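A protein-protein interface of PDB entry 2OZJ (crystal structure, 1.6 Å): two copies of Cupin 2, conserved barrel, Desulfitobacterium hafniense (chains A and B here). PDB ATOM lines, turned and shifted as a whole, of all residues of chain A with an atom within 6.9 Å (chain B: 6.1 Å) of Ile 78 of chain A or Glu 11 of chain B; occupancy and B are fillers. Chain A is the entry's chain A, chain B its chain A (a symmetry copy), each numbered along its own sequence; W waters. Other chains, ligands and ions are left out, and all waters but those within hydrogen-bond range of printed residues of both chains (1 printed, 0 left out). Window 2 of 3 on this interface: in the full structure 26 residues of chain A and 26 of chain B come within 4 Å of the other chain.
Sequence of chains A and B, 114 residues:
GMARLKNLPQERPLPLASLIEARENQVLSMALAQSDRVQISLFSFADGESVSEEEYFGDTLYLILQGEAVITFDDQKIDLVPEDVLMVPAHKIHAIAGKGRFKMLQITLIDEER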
ATOM      1  N   ALA A  69     -28.523  25.192   5.861  1.00  0.00           N
ATOM      2  CA  ALA A  69     -28.127  26.223   6.806  1.00  0.00           C
ATOM      3  C   ALA A  69     -26.794  25.846   7.451  1.00  0.00           C
ATOM      4  O   ALA A  69     -26.299  24.727   7.290  1.00  0.00           O
ATOM      5  CB  ALA A  69     -29.206  26.403   7.881  1.00  0.00           C
ATOM      6  N   VAL A  70     -26.228  26.799   8.181  1.00  0.00           N
ATOM      7  CA  VAL A  70     -24.998  26.598   8.929  1.00  0.00           C
ATOM      8  C   VAL A  70     -25.168  27.275  10.273  1.00  0.00           C
ATOM      9  O   VAL A  70     -25.645  28.415  10.331  1.00  0.00           O
ATOM     10  CB  VAL A  70     -23.774  27.216   8.216  1.00  0.00           C
ATOM     11  CG1 VAL A  70     -22.496  26.973   9.017  1.00  0.00           C
ATOM     12  CG2 VAL A  70     -23.640  26.655   6.819  1.00  0.00           C
ATOM     13  N   ILE A  71     -24.810  26.583  11.347  1.00  0.00           N
ATOM     14  CA  ILE A  71     -24.829  27.170  12.667  1.00  0.00           C
ATOM     15  C   ILE A  71     -23.411  27.331  13.162  1.00  0.00           C
ATOM     16  O   ILE A  71     -22.593  26.419  13.042  1.00  0.00           O
ATOM     17  CB  ILE A  71     -25.602  26.349  13.711  1.00  0.00           C
ATOM     18  CG1 ILE A  71     -27.048  26.214  13.313  1.00  0.00           C
ATOM     19  CG2 ILE A  71     -25.575  27.066  15.037  1.00  0.00           C
ATOM     20  CD1 ILE A  71     -27.926  25.414  14.368  1.00  0.00           C
ATOM     21  N   THR A  72     -23.126  28.504  13.723  1.00  0.00           N
ATOM     22  CA  THR A  72     -21.787  28.844  14.221  1.00  0.00           C
ATOM     23  C   THR A  72     -21.790  29.044  15.727  1.00  0.00           C
ATOM     24  O   THR A  72     -22.619  29.799  16.218  1.00  0.00           O
ATOM     25  CB  THR A  72     -21.304  30.184  13.581  1.00  0.00           C
ATOM     26  OG1 THR A  72     -21.157  30.013  12.171  1.00  0.00           O
ATOM     27  CG2 THR A  72     -19.977  30.628  14.153  1.00  0.00           C
ATOM     28  N   PHE A  73     -20.850  28.412  16.447  1.00  0.00           N
ATOM     29  CA  PHE A  73     -20.652  28.687  17.893  1.00  0.00           C
ATOM     30  C   PHE A  73     -19.319  28.251  18.443  1.00  0.00           C
ATOM     31  O   PHE A  73     -18.982  27.068  18.371  1.00  0.00           O
ATOM     32  CB  PHE A  73     -21.757  28.099  18.798  1.00  0.00           C
ATOM     33  CG  PHE A  73     -22.328  26.790  18.337  1.00  0.00           C
ATOM     34  CD1 PHE A  73     -21.587  25.881  17.596  1.00  0.00           C
ATOM     35  CD2 PHE A  73     -23.627  26.466  18.673  1.00  0.00           C
ATOM     36  CE1 PHE A  73     -22.131  24.703  17.188  1.00  0.00           C
ATOM     37  CE2 PHE A  73     -24.175  25.284  18.263  1.00  0.00           C
ATOM     38  CZ  PHE A  73     -23.426  24.396  17.521  1.00  0.00           C
ATOM     39  N   GLN A  76     -16.743  26.107  15.998  1.00  0.00           N
ATOM     40  CA  GLN A  76     -17.309  25.262  14.958  1.00  0.00           C
ATOM     41  C   GLN A  76     -18.342  25.911  14.090  1.00  0.00           C
ATOM     42  O   GLN A  76     -19.096  26.731  14.555  1.00  0.00           O
ATOM     43  CB  GLN A  76     -18.023  24.093  15.615  1.00  0.00           C
ATOM     44  CG  GLN A  76     -17.102  23.030  16.108  1.00  0.00           C
ATOM     45  CD  GLN A  76     -17.888  21.791  16.440  1.00  0.00           C
ATOM     46  OE1 GLN A  76     -18.805  21.832  17.263  1.00  0.00           O
ATOM     47  NE2 GLN A  76     -17.564  20.692  15.774  1.00  0.00           N
ATOM     48  N   LYS A  77     -18.343  25.504  12.825  1.00  0.00           N
ATOM     49  CA  LYS A  77     -19.441  25.709  11.900  1.00  0.00           C
ATOM     50  C   LYS A  77     -20.060  24.328  11.681  1.00  0.00           C
ATOM     51  O   LYS A  77     -19.373  23.384  11.274  1.00  0.00           O
ATOM     52  CB  LYS A  77     -18.936  26.311  10.573  1.00  0.00           C
ATOM     53  N   ILE A  78     -21.343  24.203  11.998  1.00  0.00           N
ATOM     54  CA  ILE A  78     -22.094  22.969  11.800  1.00  0.00           C
ATOM     55  C   ILE A  78     -23.078  23.182  10.650  1.00  0.00           C
ATOM     56  O   ILE A  78     -23.904  24.083  10.698  1.00  0.00           O
ATOM     57  CB  ILE A  78     -22.872  22.592  13.064  1.00  0.00           C
ATOM     58  CG1 ILE A  78     -21.910  22.190  14.181  1.00  0.00           C
ATOM     59  CG2 ILE A  78     -23.857  21.463  12.773  1.00  0.00           C
ATOM     60  CD1 ILE A  78     -22.604  21.888  15.494  1.00  0.00           C
ATOM     61  N   ASP A  79     -22.966  22.340   9.629  1.00  0.00           N
ATOM     62  CA  ASP A  79     -23.837  22.351   8.462  1.00  0.00           C
ATOM     63  C   ASP A  79     -25.100  21.523   8.717  1.00  0.00           C
ATOM     64  O   ASP A  79     -25.048  20.441   9.322  1.00  0.00           O
ATOM     65  CB  ASP A  79     -23.112  21.773   7.236  1.00  0.00           C
ATOM     66  CG  ASP A  79     -21.946  22.627   6.780  1.00  0.00           C
ATOM     67  OD1 ASP A  79     -22.070  23.870   6.772  1.00  0.00           O
ATOM     68  OD2 ASP A  79     -20.916  22.030   6.422  1.00  0.00           O
ATOM     69  N   LEU A  80     -26.211  22.023   8.195  1.00  0.00           N
ATOM     70  CA  LEU A  80     -27.508  21.378   8.339  1.00  0.00           C
ATOM     71  C   LEU A  80     -28.218  21.249   6.995  1.00  0.00           C
ATOM     72  O   LEU A  80     -28.092  22.120   6.104  1.00  0.00           O
ATOM     73  CB  LEU A  80     -28.395  22.133   9.334  1.00  0.00           C
ATOM     74  CG  LEU A  80     -27.922  22.182  10.802  1.00  0.00           C
ATOM     75  CD1 LEU A  80     -27.270  23.541  11.064  1.00  0.00           C
ATOM     76  CD2 LEU A  80     -29.051  21.938  11.806  1.00  0.00           C
ATOM     77  N   LEU A  86     -30.991  20.062  15.591  1.00  0.00           N
ATOM     78  CA  LEU A  86     -29.882  20.341  16.496  1.00  0.00           C
ATOM     79  C   LEU A  86     -30.414  21.095  17.695  1.00  0.00           C
ATOM     80  O   LEU A  86     -31.216  22.012  17.531  1.00  0.00           O
ATOM     81  CB  LEU A  86     -28.794  21.184  15.807  1.00  0.00           C
ATOM     82  CG  LEU A  86     -27.420  21.187  16.508  1.00  0.00           C
ATOM     83  CD1 LEU A  86     -26.678  19.834  16.473  1.00  0.00           C
ATOM     84  CD2 LEU A  86     -26.524  22.243  15.886  1.00  0.00           C
ATOM     85  N   MET A  87     -29.985  20.698  18.891  1.00  0.00           N
ATOM     86  CA  MET A  87     -30.337  21.384  20.118  1.00  0.00           C
ATOM     87  C   MET A  87     -29.168  22.249  20.550  1.00  0.00           C
ATOM     88  O   MET A  87     -28.028  21.788  20.602  1.00  0.00           O
ATOM     89  CB  MET A  87     -30.672  20.383  21.220  1.00  0.00           C
ATOM     90  CG  MET A  87     -31.429  21.020  22.404  1.00  0.00           C
ATOM     91  SD  MET A  87     -30.304  21.797  23.721  1.00  0.00           S
ATOM     92  CE  MET A  87     -30.151  20.371  25.002  1.00  0.00           C
ATOM     93  N   PRO B   9     -29.467  15.716  19.463  1.00  0.00           N
ATOM     94  CA  PRO B   9     -28.045  16.002  19.237  1.00  0.00           C
ATOM     95  C   PRO B   9     -27.664  17.468  19.419  1.00  0.00           C
ATOM     96  O   PRO B   9     -28.460  18.368  19.089  1.00  0.00           O
ATOM     97  CB  PRO B   9     -27.823  15.574  17.792  1.00  0.00           C
ATOM     98  CG  PRO B   9     -29.125  15.518  17.149  1.00  0.00           C
ATOM     99  CD  PRO B   9     -30.174  15.360  18.215  1.00  0.00           C
ATOM    100  N   GLN B  10     -26.474  17.703  19.976  1.00  0.00           N
ATOM    101  CA  GLN B  10     -25.974  19.038  20.184  1.00  0.00           C
ATOM    102  C   GLN B  10     -24.739  19.320  19.370  1.00  0.00           C
ATOM    103  O   GLN B  10     -24.398  20.490  19.176  1.00  0.00           O
ATOM    104  CB  GLN B  10     -25.653  19.259  21.650  1.00  0.00           C
ATOM    105  CG  GLN B  10     -26.875  19.249  22.544  1.00  0.00           C
ATOM    106  CD  GLN B  10     -26.508  19.415  23.985  1.00  0.00           C
ATOM    107  OE1 GLN B  10     -25.584  20.162  24.314  1.00  0.00           O
ATOM    108  NE2 GLN B  10     -27.191  18.684  24.862  1.00  0.00           N
ATOM    109  N   GLU B  11     -24.050  18.282  18.902  1.00  0.00           N
ATOM    110  CA  GLU B  11     -22.849  18.512  18.122  1.00  0.00           C
ATOM    111  C   GLU B  11     -22.894  18.000  16.689  1.00  0.00           C
ATOM    112  O   GLU B  11     -22.170  18.523  15.859  1.00  0.00           O
ATOM    113  CB  GLU B  11     -21.630  17.901  18.813  1.00  0.00           C
ATOM    114  CG  GLU B  11     -21.770  17.763  20.331  1.00  0.00           C
ATOM    115  CD  GLU B  11     -20.459  17.817  21.048  1.00  0.00           C
ATOM    116  OE1 GLU B  11     -19.565  18.605  20.622  1.00  0.00           O
ATOM    117  OE2 GLU B  11     -20.302  17.054  22.041  1.00  0.00           O
ATOM    118  N   ARG B  12     -23.648  16.934  16.417  1.00  0.00           N
ATOM    119  CA  ARG B  12     -23.817  16.489  15.031  1.00  0.00           C
ATOM    120  C   ARG B  12     -25.309  16.352  14.754  1.00  0.00           C
ATOM    121  O   ARG B  12     -25.972  15.556  15.377  1.00  0.00           O
ATOM    122  CB  ARG B  12     -22.998  15.213  14.726  1.00  0.00           C
ATOM    123  CG  ARG B  12     -23.720  14.031  14.005  1.00  0.00           C
ATOM    124  CD  ARG B  12     -22.806  12.790  13.969  1.00  0.00           C
ATOM    125  NE  ARG B  12     -21.527  13.099  13.299  1.00  0.00           N
ATOM    126  CZ  ARG B  12     -20.507  12.261  13.237  1.00  0.00           C
ATOM    127  NH1 ARG B  12     -20.717  11.095  13.790  1.00  0.00           N
ATOM    128  NH2 ARG B  12     -19.374  12.612  12.601  1.00  0.00           N
ATOM    129  N   PRO B  13     -25.827  17.154  13.825  1.00  0.00           N
ATOM    130  CA  PRO B  13     -27.246  17.120  13.510  1.00  0.00           C
ATOM    131  C   PRO B  13     -27.645  15.767  12.919  1.00  0.00           C
ATOM    132  O   PRO B  13     -26.822  15.102  12.239  1.00  0.00           O
ATOM    133  CB  PRO B  13     -27.388  18.235  12.471  1.00  0.00           C
ATOM    134  CG  PRO B  13     -26.077  18.297  11.811  1.00  0.00           C
ATOM    135  CD  PRO B  13     -25.093  18.055  12.917  1.00  0.00           C
HETATM  136  O   HOH W   1     -25.501  22.573  20.175  1.00  0.00           O
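Among the printed residues, pairs that only touch across the chains: Met 87 of chain A with Gln 10 of chain B (3.4 Å), Ile 78 of chain A with Glu 11 of chain B (3.4 Å), Asp 79 of chain A with Pro 13 of chain B (3.4 Å), Leu 86 of chain A with Pro 9 of chain B (3.5 Å), Leu 86 of chain A with Gln 10 of chain B (3.5 Å), Ile 78 of chain A with Pro 13 of chain B (3.6 Å), Leu 86 of chain A with Pro 13 of chain B (3.9 Å) and Leu 86 of chain A with Glu 11 of chain B (3.9 Å).
O of Ile 78 of chain A lies within hydrogen-bond range of N of Ile 71 of chain A (2.7 Å).
Hydrophobic or aromatic side chains of chain B that line the printed part of chain A: Pro 13.
Along chain B the printed residues that touch a printed residue of chain A span positions 9 to 13.
Hydrophobic or aromatic side chains of chain A that line the printed part of chain B: Ile 78, Leu 86 and Met 87.
Among the printed residues, 9 pairs touch across the chains.
Glu 11 of chain B touches just these residues of chain A: Ile 78 (3.4 Å) and Leu 86 (3.9 Å).
Of the printed residues of chain A, Pro 9 of chain B touches Leu 86 (3.5 Å) and Met 87 (2.8 Å).
Printed residues of chain B within 4 Å of Asp 79 of chain A: Pro 13 (3.4 Å).
The nearest printed residue of chain B that does not touch Asp 79 of chain A is Arg 12 of chain B (6.8 Å).
Water W1 lies within hydrogen-bond range of the backbone carbonyl oxygen of Gln 10 of chain B (2.6 Å) and the backbone carbonyl oxygen of Met 87 of chain A (2.7 Å).
The backbone NH of Met 87 of chain A lies within hydrogen-bond range of the backbone carbonyl oxygen of Pro 9 of chain B (2.8 Å).
No position is printed for both chains.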
